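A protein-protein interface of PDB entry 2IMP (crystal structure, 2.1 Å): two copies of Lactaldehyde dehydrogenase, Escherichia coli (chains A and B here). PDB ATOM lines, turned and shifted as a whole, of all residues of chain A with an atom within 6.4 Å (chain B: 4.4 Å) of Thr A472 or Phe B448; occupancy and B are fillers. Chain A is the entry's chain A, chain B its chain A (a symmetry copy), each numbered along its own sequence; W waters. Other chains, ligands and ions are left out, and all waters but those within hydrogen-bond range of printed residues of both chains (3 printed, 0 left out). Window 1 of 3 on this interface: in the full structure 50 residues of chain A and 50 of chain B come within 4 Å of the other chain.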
ATOM      1  N   GLU A 125     -21.802 -20.766   7.825  1.00  0.00           N
ATOM      2  CA  GLU A 125     -23.232 -20.559   7.658  1.00  0.00           C
ATOM      3  C   GLU A 125     -23.973 -21.707   6.970  1.00  0.00           C
ATOM      4  O   GLU A 125     -23.386 -22.489   6.228  1.00  0.00           O
ATOM      5  CB  GLU A 125     -23.476 -19.276   6.852  1.00  0.00           C
ATOM      6  CG  GLU A 125     -22.650 -18.087   7.321  1.00  0.00           C
ATOM      7  CD  GLU A 125     -22.377 -17.081   6.216  1.00  0.00           C
ATOM      8  OE1 GLU A 125     -22.046 -17.502   5.088  1.00  0.00           O
ATOM      9  OE2 GLU A 125     -22.480 -15.868   6.479  1.00  0.00           O
ATOM     10  N   ILE A 127     -27.040 -22.230   4.455  1.00  0.00           N
ATOM     11  CA  ILE A 127     -27.873 -21.535   3.490  1.00  0.00           C
ATOM     12  C   ILE A 127     -28.995 -22.353   2.848  1.00  0.00           C
ATOM     13  O   ILE A 127     -28.776 -23.479   2.401  1.00  0.00           O
ATOM     14  CB  ILE A 127     -26.982 -20.972   2.358  1.00  0.00           C
ATOM     15  CG1 ILE A 127     -25.865 -20.117   2.964  1.00  0.00           C
ATOM     16  CG2 ILE A 127     -27.812 -20.156   1.378  1.00  0.00           C
ATOM     17  CD1 ILE A 127     -24.710 -19.852   2.002  1.00  0.00           C
ATOM     18  N   LEU A 138     -21.687 -23.648   4.402  1.00  0.00           N
ATOM     19  CA  LEU A 138     -20.551 -22.775   4.181  1.00  0.00           C
ATOM     20  C   LEU A 138     -19.590 -22.751   5.389  1.00  0.00           C
ATOM     21  O   LEU A 138     -19.868 -22.130   6.420  1.00  0.00           O
ATOM     22  CB  LEU A 138     -21.037 -21.357   3.840  1.00  0.00           C
ATOM     23  CG  LEU A 138     -19.977 -20.306   3.494  1.00  0.00           C
ATOM     24  CD1 LEU A 138     -20.568 -19.260   2.547  1.00  0.00           C
ATOM     25  CD2 LEU A 138     -19.461 -19.650   4.781  1.00  0.00           C
ATOM     26  N   PHE A 139     -18.486 -23.472   5.256  1.00  0.00           N
ATOM     27  CA  PHE A 139     -17.495 -23.534   6.317  1.00  0.00           C
ATOM     28  C   PHE A 139     -16.402 -22.471   6.195  1.00  0.00           C
ATOM     29  O   PHE A 139     -16.048 -22.052   5.092  1.00  0.00           O
ATOM     30  CB  PHE A 139     -16.781 -24.889   6.331  1.00  0.00           C
ATOM     31  CG  PHE A 139     -17.679 -26.069   6.551  1.00  0.00           C
ATOM     32  CD1 PHE A 139     -18.382 -26.634   5.493  1.00  0.00           C
ATOM     33  CD2 PHE A 139     -17.777 -26.655   7.813  1.00  0.00           C
ATOM     34  CE1 PHE A 139     -19.152 -27.779   5.677  1.00  0.00           C
ATOM     35  CE2 PHE A 139     -18.547 -27.800   8.010  1.00  0.00           C
ATOM     36  CZ  PHE A 139     -19.239 -28.363   6.939  1.00  0.00           C
ATOM     37  N   LYS A 140     -15.878 -22.050   7.338  1.00  0.00           N
ATOM     38  CA  LYS A 140     -14.780 -21.095   7.372  1.00  0.00           C
ATOM     39  C   LYS A 140     -13.457 -21.843   7.619  1.00  0.00           C
ATOM     40  O   LYS A 140     -13.253 -22.407   8.693  1.00  0.00           O
ATOM     41  CB  LYS A 140     -15.003 -20.068   8.486  1.00  0.00           C
ATOM     42  CG  LYS A 140     -16.176 -19.129   8.247  1.00  0.00           C
ATOM     43  CD  LYS A 140     -15.941 -18.287   7.001  1.00  0.00           C
ATOM     44  CE  LYS A 140     -17.051 -17.271   6.807  1.00  0.00           C
ATOM     45  NZ  LYS A 140     -17.208 -16.407   8.005  1.00  0.00           N
ATOM     46  N   ARG A 141     -12.589 -21.872   6.616  1.00  0.00           N
ATOM     47  CA  ARG A 141     -11.316 -22.572   6.737  1.00  0.00           C
ATOM     48  C   ARG A 141     -10.107 -21.635   6.764  1.00  0.00           C
ATOM     49  O   ARG A 141     -10.197 -20.490   6.332  1.00  0.00           O
ATOM     50  CB  ARG A 141     -11.122 -23.540   5.561  1.00  0.00           C
ATOM     51  CG  ARG A 141     -12.299 -24.446   5.240  1.00  0.00           C
ATOM     52  CD  ARG A 141     -12.592 -25.421   6.361  1.00  0.00           C
ATOM     53  NE  ARG A 141     -13.479 -26.490   5.910  1.00  0.00           N
ATOM     54  CZ  ARG A 141     -14.084 -27.361   6.716  1.00  0.00           C
ATOM     55  NH1 ARG A 141     -13.907 -27.293   8.030  1.00  0.00           N
ATOM     56  NH2 ARG A 141     -14.865 -28.305   6.206  1.00  0.00           N
ATOM     57  N   LEU A 470      -9.465 -16.011   7.005  1.00  0.00           N
ATOM     58  CA  LEU A 470     -10.342 -17.128   6.740  1.00  0.00           C
ATOM     59  C   LEU A 470     -10.869 -17.122   5.308  1.00  0.00           C
ATOM     60  O   LEU A 470     -11.003 -16.073   4.693  1.00  0.00           O
ATOM     61  CB  LEU A 470     -11.534 -17.093   7.700  1.00  0.00           C
ATOM     62  CG  LEU A 470     -11.252 -17.392   9.174  1.00  0.00           C
ATOM     63  CD1 LEU A 470     -12.428 -16.929  10.033  1.00  0.00           C
ATOM     64  CD2 LEU A 470     -10.994 -18.888   9.343  1.00  0.00           C
ATOM     65  N   GLN A 471     -11.114 -18.307   4.781  1.00  0.00           N
ATOM     66  CA  GLN A 471     -11.690 -18.439   3.463  1.00  0.00           C
ATOM     67  C   GLN A 471     -12.835 -19.444   3.513  1.00  0.00           C
ATOM     68  O   GLN A 471     -12.895 -20.282   4.414  1.00  0.00           O
ATOM     69  CB  GLN A 471     -10.643 -18.848   2.419  1.00  0.00           C
ATOM     70  CG  GLN A 471     -10.014 -20.212   2.610  1.00  0.00           C
ATOM     71  CD  GLN A 471      -8.868 -20.437   1.633  1.00  0.00           C
ATOM     72  OE1 GLN A 471      -8.794 -19.786   0.584  1.00  0.00           O
ATOM     73  NE2 GLN A 471      -7.976 -21.363   1.966  1.00  0.00           N
ATOM     74  N   THR A 472     -13.732 -19.358   2.551  1.00  0.00           N
ATOM     75  CA  THR A 472     -14.887 -20.221   2.571  1.00  0.00           C
ATOM     76  C   THR A 472     -14.824 -21.496   1.742  1.00  0.00           C
ATOM     77  O   THR A 472     -14.181 -21.560   0.695  1.00  0.00           O
ATOM     78  CB  THR A 472     -16.134 -19.442   2.122  1.00  0.00           C
ATOM     79  OG1 THR A 472     -15.932 -18.961   0.787  1.00  0.00           O
ATOM     80  CG2 THR A 472     -16.375 -18.253   3.039  1.00  0.00           C
ATOM     81  N   GLN A 473     -15.478 -22.518   2.276  1.00  0.00           N
ATOM     82  CA  GLN A 473     -15.648 -23.778   1.583  1.00  0.00           C
ATOM     83  C   GLN A 473     -17.154 -24.080   1.543  1.00  0.00           C
ATOM     84  O   GLN A 473     -17.757 -24.412   2.570  1.00  0.00           O
ATOM     85  CB  GLN A 473     -14.912 -24.946   2.260  1.00  0.00           C
ATOM     86  CG  GLN A 473     -15.320 -26.309   1.652  1.00  0.00           C
ATOM     87  CD  GLN A 473     -14.694 -27.510   2.344  1.00  0.00           C
ATOM     88  OE1 GLN A 473     -14.415 -27.473   3.541  1.00  0.00           O
ATOM     89  NE2 GLN A 473     -14.488 -28.591   1.593  1.00  0.00           N
ATOM     90  N   VAL A 474     -17.758 -23.890   0.376  1.00  0.00           N
ATOM     91  CA  VAL A 474     -19.178 -24.141   0.230  1.00  0.00           C
ATOM     92  C   VAL A 474     -19.491 -25.578  -0.185  1.00  0.00           C
ATOM     93  O   VAL A 474     -19.106 -26.033  -1.271  1.00  0.00           O
ATOM     94  CB  VAL A 474     -19.815 -23.158  -0.782  1.00  0.00           C
ATOM     95  CG1 VAL A 474     -21.305 -23.432  -0.912  1.00  0.00           C
ATOM     96  CG2 VAL A 474     -19.591 -21.725  -0.317  1.00  0.00           C
ATOM     97  N   TYR A 476     -22.223 -28.433  -1.122  1.00  0.00           N
ATOM     98  CA  TYR A 476     -23.565 -28.735  -1.581  1.00  0.00           C
ATOM     99  C   TYR A 476     -23.875 -30.219  -1.336  1.00  0.00           C
ATOM    100  O   TYR A 476     -23.524 -31.089  -2.137  1.00  0.00           O
ATOM    101  CB  TYR A 476     -23.726 -28.402  -3.068  1.00  0.00           C
ATOM    102  CG  TYR A 476     -23.612 -26.929  -3.405  1.00  0.00           C
ATOM    103  CD1 TYR A 476     -22.369 -26.313  -3.528  1.00  0.00           C
ATOM    104  CD2 TYR A 476     -24.753 -26.152  -3.626  1.00  0.00           C
ATOM    105  CE1 TYR A 476     -22.259 -24.962  -3.872  1.00  0.00           C
ATOM    106  CE2 TYR A 476     -24.653 -24.799  -3.966  1.00  0.00           C
ATOM    107  CZ  TYR A 476     -23.400 -24.213  -4.087  1.00  0.00           C
ATOM    108  OH  TYR A 476     -23.289 -22.880  -4.425  1.00  0.00           O
ATOM    109  N   PHE B 432     -10.842 -26.808  -1.392  1.00  0.00           N
ATOM    110  CA  PHE B 432     -11.511 -26.090  -2.467  1.00  0.00           C
ATOM    111  C   PHE B 432     -12.617 -25.128  -1.983  1.00  0.00           C
ATOM    112  O   PHE B 432     -13.182 -25.313  -0.906  1.00  0.00           O
ATOM    113  CB  PHE B 432     -12.116 -27.095  -3.462  1.00  0.00           C
ATOM    114  CG  PHE B 432     -11.093 -27.919  -4.197  1.00  0.00           C
ATOM    115  CD1 PHE B 432     -10.379 -28.918  -3.541  1.00  0.00           C
ATOM    116  CD2 PHE B 432     -10.797 -27.651  -5.530  1.00  0.00           C
ATOM    117  CE1 PHE B 432      -9.397 -29.642  -4.207  1.00  0.00           C
ATOM    118  CE2 PHE B 432      -9.813 -28.373  -6.203  1.00  0.00           C
ATOM    119  CZ  PHE B 432      -9.108 -29.361  -5.539  1.00  0.00           C
ATOM    120  N   GLY B 433     -12.909 -24.109  -2.783  1.00  0.00           N
ATOM    121  CA  GLY B 433     -13.939 -23.154  -2.411  1.00  0.00           C
ATOM    122  C   GLY B 433     -15.319 -23.781  -2.475  1.00  0.00           C
ATOM    123  O   GLY B 433     -16.279 -23.260  -1.901  1.00  0.00           O
ATOM    124  N   GLU B 434     -15.415 -24.902  -3.182  1.00  0.00           N
ATOM    125  CA  GLU B 434     -16.673 -25.619  -3.326  1.00  0.00           C
ATOM    126  C   GLU B 434     -16.519 -27.151  -3.405  1.00  0.00           C
ATOM    127  O   GLU B 434     -15.593 -27.669  -4.038  1.00  0.00           O
ATOM    128  CB  GLU B 434     -17.416 -25.161  -4.588  1.00  0.00           C
ATOM    129  CG  GLU B 434     -17.706 -23.676  -4.674  1.00  0.00           C
ATOM    130  CD  GLU B 434     -18.357 -23.297  -5.995  1.00  0.00           C
ATOM    131  OE1 GLU B 434     -18.032 -23.933  -7.023  1.00  0.00           O
ATOM    132  OE2 GLU B 434     -19.179 -22.359  -6.006  1.00  0.00           O
ATOM    133  N   GLY B 447     -25.077 -18.908  -2.974  1.00  0.00           N
ATOM    134  CA  GLY B 447     -23.865 -19.483  -2.412  1.00  0.00           C
ATOM    135  C   GLY B 447     -22.719 -18.489  -2.506  1.00  0.00           C
ATOM    136  O   GLY B 447     -22.931 -17.277  -2.537  1.00  0.00           O
ATOM    137  N   PHE B 448     -21.493 -18.990  -2.525  1.00  0.00           N
ATOM    138  CA  PHE B 448     -20.330 -18.126  -2.655  1.00  0.00           C
ATOM    139  C   PHE B 448     -19.247 -18.784  -3.523  1.00  0.00           C
ATOM    140  O   PHE B 448     -18.513 -19.666  -3.076  1.00  0.00           O
ATOM    141  CB  PHE B 448     -19.760 -17.747  -1.272  1.00  0.00           C
ATOM    142  CG  PHE B 448     -18.707 -16.646  -1.316  1.00  0.00           C
ATOM    143  CD1 PHE B 448     -18.863 -15.537  -2.152  1.00  0.00           C
ATOM    144  CD2 PHE B 448     -17.584 -16.698  -0.489  1.00  0.00           C
ATOM    145  CE1 PHE B 448     -17.919 -14.498  -2.168  1.00  0.00           C
ATOM    146  CE2 PHE B 448     -16.633 -15.670  -0.492  1.00  0.00           C
ATOM    147  CZ  PHE B 448     -16.802 -14.560  -1.336  1.00  0.00           C
ATOM    148  N   HIS B 449     -19.224 -18.381  -4.787  1.00  0.00           N
ATOM    149  CA  HIS B 449     -18.258 -18.879  -5.751  1.00  0.00           C
ATOM    150  C   HIS B 449     -16.908 -18.158  -5.580  1.00  0.00           C
ATOM    151  O   HIS B 449     -16.703 -17.062  -6.107  1.00  0.00           O
ATOM    152  CB  HIS B 449     -18.786 -18.648  -7.165  1.00  0.00           C
ATOM    153  CG  HIS B 449     -18.099 -19.462  -8.220  1.00  0.00           C
ATOM    154  ND1 HIS B 449     -18.133 -20.845  -8.227  1.00  0.00           N
ATOM    155  CD2 HIS B 449     -17.431 -19.096  -9.334  1.00  0.00           C
ATOM    156  CE1 HIS B 449     -17.516 -21.287  -9.308  1.00  0.00           C
ATOM    157  NE2 HIS B 449     -17.081 -20.249  -9.997  1.00  0.00           N
ATOM    158  N   ALA B 450     -16.026 -18.776  -4.802  1.00  0.00           N
ATOM    159  CA  ALA B 450     -14.713 -18.221  -4.519  1.00  0.00           C
ATOM    160  C   ALA B 450     -13.616 -19.301  -4.550  1.00  0.00           C
ATOM    161  O   ALA B 450     -13.684 -20.288  -3.825  1.00  0.00           O
ATOM    162  CB  ALA B 450     -14.732 -17.529  -3.160  1.00  0.00           C
ATOM    163  N   TRP B 452      -9.833 -21.072  -4.199  1.00  0.00           N
ATOM    164  CA  TRP B 452      -8.631 -21.113  -3.383  1.00  0.00           C
ATOM    165  C   TRP B 452      -7.374 -21.060  -4.278  1.00  0.00           C
ATOM    166  O   TRP B 452      -7.474 -21.231  -5.495  1.00  0.00           O
ATOM    167  CB  TRP B 452      -8.597 -22.406  -2.576  1.00  0.00           C
ATOM    168  CG  TRP B 452      -9.585 -22.482  -1.451  1.00  0.00           C
ATOM    169  CD1 TRP B 452     -10.816 -21.892  -1.387  1.00  0.00           C
ATOM    170  CD2 TRP B 452      -9.434 -23.234  -0.243  1.00  0.00           C
ATOM    171  NE1 TRP B 452     -11.440 -22.228  -0.210  1.00  0.00           N
ATOM    172  CE2 TRP B 452     -10.615 -23.048   0.512  1.00  0.00           C
ATOM    173  CE3 TRP B 452      -8.414 -24.038   0.279  1.00  0.00           C
ATOM    174  CZ2 TRP B 452     -10.807 -23.652   1.762  1.00  0.00           C
ATOM    175  CZ3 TRP B 452      -8.603 -24.637   1.525  1.00  0.00           C
ATOM    176  CH2 TRP B 452      -9.792 -24.435   2.251  1.00  0.00           C
ATOM    177  N   GLY B 458     -11.087 -12.968  -3.624  1.00  0.00           N
ATOM    178  CA  GLY B 458     -12.418 -12.467  -3.348  1.00  0.00           C
ATOM    179  C   GLY B 458     -13.386 -13.520  -3.863  1.00  0.00           C
ATOM    180  O   GLY B 458     -13.092 -14.719  -3.819  1.00  0.00           O
ATOM    181  N   GLY B 459     -14.533 -13.095  -4.370  1.00  0.00           N
ATOM    182  CA  GLY B 459     -15.482 -14.066  -4.871  1.00  0.00           C
ATOM    183  C   GLY B 459     -16.753 -13.438  -5.387  1.00  0.00           C
ATOM    184  O   GLY B 459     -16.880 -12.213  -5.408  1.00  0.00           O
ATOM    185  N   ALA B 460     -17.692 -14.287  -5.804  1.00  0.00           N
ATOM    186  CA  ALA B 460     -18.972 -13.827  -6.329  1.00  0.00           C
ATOM    187  C   ALA B 460     -20.200 -14.622  -5.820  1.00  0.00           C
ATOM    188  O   ALA B 460     -20.072 -15.757  -5.340  1.00  0.00           O
ATOM    189  CB  ALA B 460     -18.943 -13.854  -7.857  1.00  0.00           C
ATOM    190  N   ASP B 461     -21.367 -13.995  -5.950  1.00  0.00           N
ATOM    191  CA  ASP B 461     -22.654 -14.555  -5.550  1.00  0.00           C
ATOM    192  C   ASP B 461     -22.992 -14.437  -4.043  1.00  0.00           C
ATOM    193  O   ASP B 461     -22.109 -14.260  -3.198  1.00  0.00           O
ATOM    194  CB  ASP B 461     -22.766 -16.034  -5.951  1.00  0.00           C
ATOM    195  CG  ASP B 461     -22.349 -16.299  -7.397  1.00  0.00           C
ATOM    196  OD1 ASP B 461     -22.348 -15.367  -8.223  1.00  0.00           O
ATOM    197  OD2 ASP B 461     -22.034 -17.465  -7.712  1.00  0.00           O
ATOM    198  N   HIS B 464     -21.813 -12.753   0.492  1.00  0.00           N
ATOM    199  CA  HIS B 464     -20.391 -12.469   0.424  1.00  0.00           C
ATOM    200  C   HIS B 464     -19.966 -11.851  -0.914  1.00  0.00           C
ATOM    201  O   HIS B 464     -19.062 -11.026  -0.959  1.00  0.00           O
ATOM    202  CB  HIS B 464     -19.603 -13.744   0.719  1.00  0.00           C
ATOM    203  CG  HIS B 464     -19.929 -14.335   2.057  1.00  0.00           C
ATOM    204  ND1 HIS B 464     -19.665 -13.684   3.242  1.00  0.00           N
ATOM    205  CD2 HIS B 464     -20.565 -15.483   2.390  1.00  0.00           C
ATOM    206  CE1 HIS B 464     -20.125 -14.400   4.247  1.00  0.00           C
ATOM    207  NE2 HIS B 464     -20.678 -15.498   3.764  1.00  0.00           N
ATOM    208  N   GLY B 465     -20.639 -12.252  -1.987  1.00  0.00           N
ATOM    209  CA  GLY B 465     -20.340 -11.683  -3.291  1.00  0.00           C
ATOM    210  C   GLY B 465     -20.780 -10.231  -3.275  1.00  0.00           C
ATOM    211  O   GLY B 465     -20.104  -9.356  -3.812  1.00  0.00           O
ATOM    212  N   GLU B 468     -18.319  -7.847  -1.527  1.00  0.00           N
ATOM    213  CA  GLU B 468     -17.092  -7.495  -2.237  1.00  0.00           C
ATOM    214  C   GLU B 468     -17.181  -6.055  -2.799  1.00  0.00           C
ATOM    215  O   GLU B 468     -16.167  -5.404  -3.036  1.00  0.00           O
ATOM    216  CB  GLU B 468     -16.821  -8.459  -3.410  1.00  0.00           C
ATOM    217  CG  GLU B 468     -16.391  -9.881  -3.045  1.00  0.00           C
ATOM    218  CD  GLU B 468     -15.154  -9.932  -2.150  1.00  0.00           C
ATOM    219  OE1 GLU B 468     -14.311  -9.009  -2.227  1.00  0.00           O
ATOM    220  OE2 GLU B 468     -15.024 -10.908  -1.378  1.00  0.00           O
HETATM  221  O   HOH W   1     -16.444 -20.445  -1.467  1.00  0.00           O
HETATM  222  O   HOH W   2     -13.274 -19.425  -1.049  1.00  0.00           O
HETATM  223  O   HOH W   3     -20.994 -21.398  -4.474  1.00  0.00           O
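No position is printed for both chains. Of the 13 pairs that touch across the chains among the printed residues, none has its exchanged pair printed and touching as well.
Printed residues of chain B that touch a printed residue of chain A: Phe B432, Gly B433, Glu B434, Gly B447, Phe B448, Trp B452 and His B464. Hydrophobic or aromatic side chains of chain A within 4 Å of the printed part of chain B: Leu A138, Val A474 and Tyr A476.
The backbone carbonyl oxygen of Thr A472 lies within hydrogen-bond range of the indole nitrogen of Trp B452, at 3.0 Å. OE1 of Glu A125 is in hydrogen-bond range of NE2 of His B464, at 2.8 Å. N of Val A474 sits at hydrogen-bond distance from O of Gly B433.
Among the printed residues, merely in contact across the chains: Leu A138 with His B464 (3.8 Å), Arg A141 with Trp B452 (3.7 Å), Gln A471 with Trp B452 (3.2 Å), Thr A472 with Gly B433 (3.5 Å), Thr A472 with Phe B448 (3.1 Å), Gln A473 with Phe B432 (3.5 Å), Gln A473 with Gly B433 (3.6 Å), Val A474 with Glu B434 (3.2 Å), Val A474 with Phe B448 (3.6 Å) and Tyr A476 with Gly B447 (3.99 Å).
N of Arg A141 sits at hydrogen-bond distance from O of Gln A471, at 2.7 Å. O of Phe A139 sits at hydrogen-bond distance from N of Gln A473 (2.9 Å). O of Glu A125 lies within hydrogen-bond range of N of Leu A138. OE2 of Glu B434 is in hydrogen-bond range of ND1 of His B449, at 2.9 Å. NE of Arg A141 sits at hydrogen-bond distance from OE1 of Gln A473 (2.7 Å).
Of the printed residues of chain B, Leu A138 touches His B464 (3.8 Å). Lys A140 touches none of the printed residues of chain B. Of the printed residues of chain A, Phe B432 touches Gln A473 (3.5 Å). Of the printed residues of chain A, Gly B433 touches Thr A472 (3.5 Å), Gln A473 (3.6 Å) and Val A474 (2.8 Å). Printed residues of chain A within 4 Å of Gly B447: Tyr A476. Of chain A, only Thr A472 and Val A474 come within 4 Å of Phe B448. His B449 touches none of the printed residues of chain A. The nearest residue of chain B that does not touch Thr A472 is Phe B432 (4.2 Å). The nearest printed residue of chain A that does not touch Gly B447 is Ile A127 (4.5 Å).
Water W3 lies within hydrogen-bond range of OE2 of Glu B434 (2.6 Å), OH of Tyr A476 (2.7 Å) and N of Phe B448 (3.1 Å). Water W1 lies within hydrogen-bond range of O of Phe B448 (2.7 Å), OG1 of Thr A472 (2.7 Å) and O of Gly B433 (2.9 Å). Water W2 lies within hydrogen-bond range of O of Thr A472 (2.9 Å), O of Ala B450 (2.9 Å) and NE1 of Trp B452 (3.5 Å).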
